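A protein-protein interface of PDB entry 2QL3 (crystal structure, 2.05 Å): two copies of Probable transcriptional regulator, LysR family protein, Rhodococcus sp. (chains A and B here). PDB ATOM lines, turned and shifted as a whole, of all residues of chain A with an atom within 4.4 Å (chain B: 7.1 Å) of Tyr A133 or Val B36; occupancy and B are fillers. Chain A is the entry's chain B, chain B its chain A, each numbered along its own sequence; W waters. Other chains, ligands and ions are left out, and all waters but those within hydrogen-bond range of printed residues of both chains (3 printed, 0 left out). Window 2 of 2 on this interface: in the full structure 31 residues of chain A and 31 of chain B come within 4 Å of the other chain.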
ATOM      1  N   MET A 106     -12.512   7.473 -22.746  1.00  0.00           N
ATOM      2  CA  MET A 106     -11.219   7.242 -23.323  1.00  0.00           C
ATOM      3  C   MET A 106     -10.193   8.323 -22.958  1.00  0.00           C
ATOM      4  O   MET A 106     -10.506   9.538 -22.805  1.00  0.00           O
ATOM      5  CB  MET A 106     -11.346   7.040 -24.846  1.00  0.00           C
ATOM      6  CG  MET A 106     -10.063   6.646 -25.538  1.00  0.00           C
ATOM      7  SD  MET A 106      -9.967   6.977 -27.456  1.00  0.00           S
ATOM      8  CE  MET A 106      -8.357   5.842 -27.674  1.00  0.00           C
ATOM      9  N   VAL A 107      -8.968   7.855 -22.735  1.00  0.00           N
ATOM     10  CA  VAL A 107      -7.833   8.755 -22.622  1.00  0.00           C
ATOM     11  C   VAL A 107      -7.181   8.605 -23.996  1.00  0.00           C
ATOM     12  O   VAL A 107      -6.687   7.536 -24.312  1.00  0.00           O
ATOM     13  CB  VAL A 107      -6.886   8.340 -21.448  1.00  0.00           C
ATOM     14  CG1 VAL A 107      -5.556   9.181 -21.469  1.00  0.00           C
ATOM     15  CG2 VAL A 107      -7.608   8.472 -20.080  1.00  0.00           C
ATOM     16  N   LEU A 108      -7.278   9.651 -24.826  1.00  0.00           N
ATOM     17  CA  LEU A 108      -6.687   9.653 -26.174  1.00  0.00           C
ATOM     18  C   LEU A 108      -5.251  10.119 -26.147  1.00  0.00           C
ATOM     19  O   LEU A 108      -4.993  11.243 -25.740  1.00  0.00           O
ATOM     20  CB  LEU A 108      -7.491  10.597 -27.097  1.00  0.00           C
ATOM     21  CG  LEU A 108      -7.160  10.676 -28.600  1.00  0.00           C
ATOM     22  CD1 LEU A 108      -7.024   9.260 -29.242  1.00  0.00           C
ATOM     23  CD2 LEU A 108      -8.182  11.520 -29.375  1.00  0.00           C
ATOM     24  N   VAL A 131     -13.859  11.014 -25.564  1.00  0.00           N
ATOM     25  CA  VAL A 131     -12.509  11.378 -25.137  1.00  0.00           C
ATOM     26  C   VAL A 131     -12.654  12.212 -23.887  1.00  0.00           C
ATOM     27  O   VAL A 131     -13.130  13.344 -23.947  1.00  0.00           O
ATOM     28  CB  VAL A 131     -11.740  12.099 -26.255  1.00  0.00           C
ATOM     29  CG1 VAL A 131     -10.323  12.524 -25.782  1.00  0.00           C
ATOM     30  CG2 VAL A 131     -11.641  11.172 -27.468  1.00  0.00           C
ATOM     31  N   ALA A 132     -12.267  11.652 -22.741  1.00  0.00           N
ATOM     32  CA  ALA A 132     -12.399  12.375 -21.479  1.00  0.00           C
ATOM     33  C   ALA A 132     -11.176  13.306 -21.249  1.00  0.00           C
ATOM     34  O   ALA A 132     -11.307  14.429 -20.675  1.00  0.00           O
ATOM     35  CB  ALA A 132     -12.589  11.371 -20.299  1.00  0.00           C
ATOM     36  N   TYR A 133      -9.997  12.798 -21.658  1.00  0.00           N
ATOM     37  CA  TYR A 133      -8.688  13.438 -21.491  1.00  0.00           C
ATOM     38  C   TYR A 133      -7.831  13.180 -22.741  1.00  0.00           C
ATOM     39  O   TYR A 133      -7.959  12.126 -23.389  1.00  0.00           O
ATOM     40  CB  TYR A 133      -7.974  12.906 -20.237  1.00  0.00           C
ATOM     41  CG  TYR A 133      -8.775  13.114 -18.961  1.00  0.00           C
ATOM     42  CD1 TYR A 133      -8.780  14.355 -18.332  1.00  0.00           C
ATOM     43  CD2 TYR A 133      -9.540  12.079 -18.394  1.00  0.00           C
ATOM     44  CE1 TYR A 133      -9.480  14.580 -17.171  1.00  0.00           C
ATOM     45  CE2 TYR A 133     -10.295  12.307 -17.231  1.00  0.00           C
ATOM     46  CZ  TYR A 133     -10.256  13.563 -16.642  1.00  0.00           C
ATOM     47  OH  TYR A 133     -10.951  13.846 -15.493  1.00  0.00           O
ATOM     48  N   ARG A 134      -6.979  14.150 -23.074  1.00  0.00           N
ATOM     49  CA  ARG A 134      -6.096  14.124 -24.253  1.00  0.00           C
ATOM     50  C   ARG A 134      -4.690  14.418 -23.804  1.00  0.00           C
ATOM     51  O   ARG A 134      -4.488  15.370 -23.036  1.00  0.00           O
ATOM     52  CB  ARG A 134      -6.471  15.229 -25.256  1.00  0.00           C
ATOM     53  CG  ARG A 134      -7.394  14.809 -26.364  1.00  0.00           C
ATOM     54  CD  ARG A 134      -7.946  16.077 -27.144  1.00  0.00           C
ATOM     55  NE  ARG A 134      -8.992  15.717 -28.100  1.00  0.00           N
ATOM     56  CZ  ARG A 134      -8.752  15.409 -29.380  1.00  0.00           C
ATOM     57  NH1 ARG A 134      -9.747  15.044 -30.200  1.00  0.00           N
ATOM     58  NH2 ARG A 134      -7.500  15.449 -29.846  1.00  0.00           N
ATOM     59  N   PHE A 144      -2.878   7.940 -16.404  1.00  0.00           N
ATOM     60  CA  PHE A 144      -4.302   8.266 -16.307  1.00  0.00           C
ATOM     61  C   PHE A 144      -5.107   6.976 -16.316  1.00  0.00           C
ATOM     62  O   PHE A 144      -6.032   6.804 -15.535  1.00  0.00           O
ATOM     63  CB  PHE A 144      -4.714   9.137 -17.489  1.00  0.00           C
ATOM     64  CG  PHE A 144      -4.577  10.602 -17.217  1.00  0.00           C
ATOM     65  CD1 PHE A 144      -3.553  11.067 -16.403  1.00  0.00           C
ATOM     66  CD2 PHE A 144      -5.460  11.518 -17.755  1.00  0.00           C
ATOM     67  CE1 PHE A 144      -3.385  12.412 -16.129  1.00  0.00           C
ATOM     68  CE2 PHE A 144      -5.294  12.909 -17.448  1.00  0.00           C
ATOM     69  CZ  PHE A 144      -4.231  13.312 -16.667  1.00  0.00           C
ATOM     70  N   LEU A 149      -9.060   6.743 -14.887  1.00  0.00           N
ATOM     71  CA  LEU A 149      -9.640   7.853 -15.625  1.00  0.00           C
ATOM     72  C   LEU A 149     -10.132   7.498 -17.042  1.00  0.00           C
ATOM     73  O   LEU A 149     -10.838   8.290 -17.682  1.00  0.00           O
ATOM     74  CB  LEU A 149      -8.660   9.034 -15.657  1.00  0.00           C
ATOM     75  CG  LEU A 149      -8.429   9.643 -14.276  1.00  0.00           C
ATOM     76  CD1 LEU A 149      -7.218  10.499 -14.390  1.00  0.00           C
ATOM     77  CD2 LEU A 149      -9.644  10.469 -13.905  1.00  0.00           C
ATOM     78  N   GLY B   5     -19.516  22.323 -12.724  1.00  0.00           N
ATOM     79  CA  GLY B   5     -19.110  23.143 -13.848  1.00  0.00           C
ATOM     80  C   GLY B   5     -17.657  22.895 -14.266  1.00  0.00           C
ATOM     81  O   GLY B   5     -16.916  22.154 -13.582  1.00  0.00           O
ATOM     82  N   PRO B   6     -17.247  23.512 -15.387  1.00  0.00           N
ATOM     83  CA  PRO B   6     -15.926  23.225 -16.038  1.00  0.00           C
ATOM     84  C   PRO B   6     -14.798  23.902 -15.319  1.00  0.00           C
ATOM     85  O   PRO B   6     -14.966  25.030 -14.878  1.00  0.00           O
ATOM     86  CB  PRO B   6     -16.087  23.849 -17.421  1.00  0.00           C
ATOM     87  CG  PRO B   6     -17.087  25.003 -17.192  1.00  0.00           C
ATOM     88  CD  PRO B   6     -18.024  24.504 -16.142  1.00  0.00           C
ATOM     89  N   ILE B   7     -13.629  23.242 -15.232  1.00  0.00           N
ATOM     90  CA  ILE B   7     -12.371  23.920 -14.833  1.00  0.00           C
ATOM     91  C   ILE B   7     -11.311  23.504 -15.825  1.00  0.00           C
ATOM     92  O   ILE B   7     -11.246  22.342 -16.183  1.00  0.00           O
ATOM     93  CB  ILE B   7     -11.902  23.634 -13.341  1.00  0.00           C
ATOM     94  CG1 ILE B   7     -10.578  24.323 -13.055  1.00  0.00           C
ATOM     95  CG2 ILE B   7     -11.791  22.102 -13.015  1.00  0.00           C
ATOM     96  CD1 ILE B   7      -9.926  23.955 -11.710  1.00  0.00           C
ATOM     97  N   ALA B   8     -10.522  24.449 -16.288  1.00  0.00           N
ATOM     98  CA  ALA B   8      -9.341  24.152 -17.140  1.00  0.00           C
ATOM     99  C   ALA B   8      -8.041  24.136 -16.321  1.00  0.00           C
ATOM    100  O   ALA B   8      -7.653  25.130 -15.708  1.00  0.00           O
ATOM    101  CB  ALA B   8      -9.232  25.083 -18.360  1.00  0.00           C
ATOM    102  N   VAL B   9      -7.445  22.956 -16.282  1.00  0.00           N
ATOM    103  CA  VAL B   9      -6.197  22.686 -15.549  1.00  0.00           C
ATOM    104  C   VAL B   9      -5.034  22.406 -16.511  1.00  0.00           C
ATOM    105  O   VAL B   9      -5.069  21.482 -17.358  1.00  0.00           O
ATOM    106  CB  VAL B   9      -6.335  21.482 -14.589  1.00  0.00           C
ATOM    107  CG1 VAL B   9      -5.011  21.295 -13.767  1.00  0.00           C
ATOM    108  CG2 VAL B   9      -7.557  21.629 -13.652  1.00  0.00           C
ATOM    109  N   LEU B  20      -0.484  14.711 -11.636  1.00  0.00           N
ATOM    110  CA  LEU B  20      -1.797  14.968 -12.134  1.00  0.00           C
ATOM    111  C   LEU B  20      -2.803  13.815 -12.049  1.00  0.00           C
ATOM    112  O   LEU B  20      -3.941  14.073 -11.743  1.00  0.00           O
ATOM    113  CB  LEU B  20      -1.740  15.494 -13.538  1.00  0.00           C
ATOM    114  CG  LEU B  20      -1.695  17.014 -13.714  1.00  0.00           C
ATOM    115  CD1 LEU B  20      -3.020  17.700 -13.326  1.00  0.00           C
ATOM    116  CD2 LEU B  20      -0.509  17.579 -12.987  1.00  0.00           C
ATOM    117  N   MET B  23      -4.545  13.575  -8.554  1.00  0.00           N
ATOM    118  CA  MET B  23      -5.222  14.843  -8.343  1.00  0.00           C
ATOM    119  C   MET B  23      -6.535  14.888  -9.096  1.00  0.00           C
ATOM    120  O   MET B  23      -7.538  15.188  -8.528  1.00  0.00           O
ATOM    121  CB  MET B  23      -4.361  16.005  -8.883  1.00  0.00           C
ATOM    122  CG  MET B  23      -3.743  16.848  -7.859  1.00  0.00           C
ATOM    123  SD  MET B  23      -2.868  18.415  -8.740  1.00  0.00           S
ATOM    124  CE  MET B  23      -4.049  18.630 -10.113  1.00  0.00           C
ATOM    125  N   LEU B  24      -6.494  14.617 -10.397  1.00  0.00           N
ATOM    126  CA  LEU B  24      -7.719  14.609 -11.234  1.00  0.00           C
ATOM    127  C   LEU B  24      -8.698  13.546 -10.764  1.00  0.00           C
ATOM    128  O   LEU B  24      -9.902  13.797 -10.668  1.00  0.00           O
ATOM    129  CB  LEU B  24      -7.392  14.409 -12.733  1.00  0.00           C
ATOM    130  CG  LEU B  24      -7.166  15.713 -13.551  1.00  0.00           C
ATOM    131  CD1 LEU B  24      -7.008  16.992 -12.674  1.00  0.00           C
ATOM    132  CD2 LEU B  24      -6.155  15.590 -14.677  1.00  0.00           C
ATOM    133  N   TYR B  25      -8.184  12.355 -10.460  1.00  0.00           N
ATOM    134  CA  TYR B  25      -9.053  11.282  -9.928  1.00  0.00           C
ATOM    135  C   TYR B  25      -9.708  11.721  -8.624  1.00  0.00           C
ATOM    136  O   TYR B  25     -10.938  11.724  -8.518  1.00  0.00           O
ATOM    137  CB  TYR B  25      -8.278   9.952  -9.769  1.00  0.00           C
ATOM    138  CG  TYR B  25      -9.206   8.810  -9.487  1.00  0.00           C
ATOM    139  CD1 TYR B  25      -9.739   8.050 -10.526  1.00  0.00           C
ATOM    140  CD2 TYR B  25      -9.604   8.542  -8.199  1.00  0.00           C
ATOM    141  CE1 TYR B  25     -10.639   7.029 -10.289  1.00  0.00           C
ATOM    142  CE2 TYR B  25     -10.522   7.520  -7.939  1.00  0.00           C
ATOM    143  CZ  TYR B  25     -11.022   6.772  -9.000  1.00  0.00           C
ATOM    144  OH  TYR B  25     -11.907   5.759  -8.762  1.00  0.00           O
ATOM    145  N   PHE B  27     -10.106  14.675  -7.323  1.00  0.00           N
ATOM    146  CA  PHE B  27     -10.971  15.861  -7.457  1.00  0.00           C
ATOM    147  C   PHE B  27     -12.334  15.485  -8.030  1.00  0.00           C
ATOM    148  O   PHE B  27     -13.403  15.836  -7.451  1.00  0.00           O
ATOM    149  CB  PHE B  27     -10.256  17.015  -8.225  1.00  0.00           C
ATOM    150  CG  PHE B  27     -11.122  18.258  -8.404  1.00  0.00           C
ATOM    151  CD1 PHE B  27     -11.352  19.120  -7.338  1.00  0.00           C
ATOM    152  CD2 PHE B  27     -11.719  18.542  -9.630  1.00  0.00           C
ATOM    153  CE1 PHE B  27     -12.185  20.242  -7.494  1.00  0.00           C
ATOM    154  CE2 PHE B  27     -12.562  19.635  -9.778  1.00  0.00           C
ATOM    155  CZ  PHE B  27     -12.797  20.486  -8.721  1.00  0.00           C
ATOM    156  N   THR B  28     -12.326  14.714  -9.119  1.00  0.00           N
ATOM    157  CA  THR B  28     -13.540  14.418  -9.845  1.00  0.00           C
ATOM    158  C   THR B  28     -14.402  13.447  -9.084  1.00  0.00           C
ATOM    159  O   THR B  28     -15.620  13.444  -9.260  1.00  0.00           O
ATOM    160  CB  THR B  28     -13.283  13.929 -11.313  1.00  0.00           C
ATOM    161  OG1 THR B  28     -12.286  12.887 -11.350  1.00  0.00           O
ATOM    162  CG2 THR B  28     -12.883  15.115 -12.164  1.00  0.00           C
ATOM    163  N   ALA B  34     -18.255  18.535 -11.316  1.00  0.00           N
ATOM    164  CA  ALA B  34     -17.238  19.380 -11.923  1.00  0.00           C
ATOM    165  C   ALA B  34     -16.723  18.653 -13.138  1.00  0.00           C
ATOM    166  O   ALA B  34     -16.679  17.417 -13.132  1.00  0.00           O
ATOM    167  CB  ALA B  34     -16.072  19.622 -10.948  1.00  0.00           C
ATOM    168  N   SER B  35     -16.310  19.367 -14.180  1.00  0.00           N
ATOM    169  CA  SER B  35     -15.583  18.681 -15.254  1.00  0.00           C
ATOM    170  C   SER B  35     -14.217  19.318 -15.533  1.00  0.00           C
ATOM    171  O   SER B  35     -14.118  20.550 -15.667  1.00  0.00           O
ATOM    172  CB  SER B  35     -16.430  18.564 -16.529  1.00  0.00           C
ATOM    173  OG  SER B  35     -16.750  19.813 -17.095  1.00  0.00           O
ATOM    174  N   VAL B  36     -13.164  18.499 -15.606  1.00  0.00           N
ATOM    175  CA  VAL B  36     -11.836  19.060 -15.889  1.00  0.00           C
ATOM    176  C   VAL B  36     -11.401  19.072 -17.330  1.00  0.00           C
ATOM    177  O   VAL B  36     -11.491  18.059 -18.042  1.00  0.00           O
ATOM    178  CB  VAL B  36     -10.723  18.618 -14.897  1.00  0.00           C
ATOM    179  CG1 VAL B  36     -11.138  17.495 -14.020  1.00  0.00           C
ATOM    180  CG2 VAL B  36      -9.317  18.535 -15.551  1.00  0.00           C
ATOM    181  N   GLU B  37     -10.960  20.244 -17.778  1.00  0.00           N
ATOM    182  CA  GLU B  37     -10.362  20.322 -19.110  1.00  0.00           C
ATOM    183  C   GLU B  37      -8.858  20.299 -18.909  1.00  0.00           C
ATOM    184  O   GLU B  37      -8.275  21.270 -18.426  1.00  0.00           O
ATOM    185  CB  GLU B  37     -10.852  21.570 -19.874  1.00  0.00           C
ATOM    186  CG  GLU B  37     -12.365  21.458 -20.304  1.00  0.00           C
ATOM    187  CD  GLU B  37     -13.342  22.499 -19.654  1.00  0.00           C
ATOM    188  OE1 GLU B  37     -13.169  23.730 -19.873  1.00  0.00           O
ATOM    189  OE2 GLU B  37     -14.304  22.063 -18.943  1.00  0.00           O
ATOM    190  N   PHE B  38      -8.250  19.173 -19.233  1.00  0.00           N
ATOM    191  CA  PHE B  38      -6.851  18.971 -18.934  1.00  0.00           C
ATOM    192  C   PHE B  38      -6.012  19.272 -20.168  1.00  0.00           C
ATOM    193  O   PHE B  38      -6.289  18.734 -21.243  1.00  0.00           O
ATOM    194  CB  PHE B  38      -6.635  17.531 -18.476  1.00  0.00           C
ATOM    195  CG  PHE B  38      -5.207  17.159 -18.326  1.00  0.00           C
ATOM    196  CD1 PHE B  38      -4.574  16.332 -19.289  1.00  0.00           C
ATOM    197  CD2 PHE B  38      -4.458  17.648 -17.261  1.00  0.00           C
ATOM    198  CE1 PHE B  38      -3.216  15.974 -19.138  1.00  0.00           C
ATOM    199  CE2 PHE B  38      -3.093  17.284 -17.116  1.00  0.00           C
ATOM    200  CZ  PHE B  38      -2.479  16.457 -18.062  1.00  0.00           C
ATOM    201  N   ARG B  39      -4.990  20.109 -20.010  1.00  0.00           N
ATOM    202  CA  ARG B  39      -4.033  20.408 -21.094  1.00  0.00           C
ATOM    203  C   ARG B  39      -2.622  20.358 -20.558  1.00  0.00           C
ATOM    204  O   ARG B  39      -2.312  21.025 -19.619  1.00  0.00           O
ATOM    205  CB  ARG B  39      -4.222  21.810 -21.720  1.00  0.00           C
ATOM    206  CG  ARG B  39      -5.627  22.330 -21.774  1.00  0.00           C
ATOM    207  CD  ARG B  39      -6.015  22.874 -23.149  1.00  0.00           C
ATOM    208  NE  ARG B  39      -7.448  23.155 -23.149  1.00  0.00           N
ATOM    209  CZ  ARG B  39      -8.411  22.250 -23.375  1.00  0.00           C
ATOM    210  NH1 ARG B  39      -8.107  20.971 -23.666  1.00  0.00           N
ATOM    211  NH2 ARG B  39      -9.692  22.627 -23.301  1.00  0.00           N
ATOM    212  N   PHE B 201     -10.974  23.605  -6.421  1.00  0.00           N
ATOM    213  CA  PHE B 201      -9.807  22.823  -6.867  1.00  0.00           C
ATOM    214  C   PHE B 201      -8.515  23.137  -6.059  1.00  0.00           C
ATOM    215  O   PHE B 201      -7.847  22.222  -5.547  1.00  0.00           O
ATOM    216  CB  PHE B 201      -9.554  22.977  -8.370  1.00  0.00           C
ATOM    217  CG  PHE B 201      -8.447  22.144  -8.872  1.00  0.00           C
ATOM    218  CD1 PHE B 201      -8.698  20.864  -9.323  1.00  0.00           C
ATOM    219  CD2 PHE B 201      -7.131  22.633  -8.945  1.00  0.00           C
ATOM    220  CE1 PHE B 201      -7.695  20.060  -9.831  1.00  0.00           C
ATOM    221  CE2 PHE B 201      -6.109  21.810  -9.443  1.00  0.00           C
ATOM    222  CZ  PHE B 201      -6.414  20.491  -9.873  1.00  0.00           C
HETATM  223  O   HOH W   1     -10.111  17.067 -20.379  1.00  0.00           O
HETATM  224  O   HOH W   2     -13.578  15.679 -15.839  1.00  0.00           O
HETATM  225  O   HOH W   3      -7.764  16.636 -21.997  1.00  0.00           O
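Water W3 bridges the backbone carbonyl oxygen (O) of Phe B38 and the backbone NH (N) of Arg A134.
Water W2 bridges the backbone NH (N) of Val B36 (2.9 Å) and the side-chain hydroxyl (OH) of Tyr A133 (3.2 Å).
Water W1 lies within hydrogen-bond range of the backbone carbonyl oxygen (O) of Val B36 (2.9 Å), the backbone carbonyl oxygen (O) of Ala A132 (2.9 Å) and the backbone NH (N) of Phe B38 (3.0 Å).
Val B36 touches just one residue of chain A: Tyr A133 (3.9 Å).
Of the printed residues of chain A, Phe B38 touches Tyr A133, Arg A134 and Phe A144.
Of the printed residues of chain B, Phe A144 touches Leu B24 (3.6 Å) and Phe B38 (3.8 Å).
Printed residues of chain B within 4 Å of Arg A134: Phe B38.
Of the printed residues of chain A, Leu B24 touches Phe A144 (3.6 Å).
Ser B35 touches none of the printed residues of chain A.
The nearest printed residue of chain A that does not touch Val B36 is Ala A132 (4.5 Å).
No position is printed for both chains.
Hydrophobic or aromatic side chains of chain A that line the printed part of chain B: Tyr A133 and Phe A144.
Of the 18 printed residues of chain B, 3 touch a printed residue of chain A.
Printed residues of chain B that touch a printed residue of chain A: Leu B24, Val B36 and Phe B38.
Among the printed residues, 5 pairs touch across the chains.
Among the printed residues, pairs that only touch across the chains: Tyr A133 with Val B36 (3.9 Å), Tyr A133 with Phe B38 (3.8 Å), Arg A134 with Phe B38 (3.9 Å), Phe A144 with Leu B24 (3.6 Å) and Phe A144 with Phe B38 (3.8 Å).
O of Leu B24 is in hydrogen-bond range of OG1 of Thr B28 (2.6 Å).
The backbone NH of Tyr A133 lies within hydrogen-bond range of the backbone carbonyl oxygen of Met A106.
O of Tyr A133 is in hydrogen-bond range of N of Leu A108 (2.9 Å).
The backbone carbonyl oxygen (O) of Phe A144 is in hydrogen-bond range of the backbone NH (N) of Leu A149 (3.1 Å).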
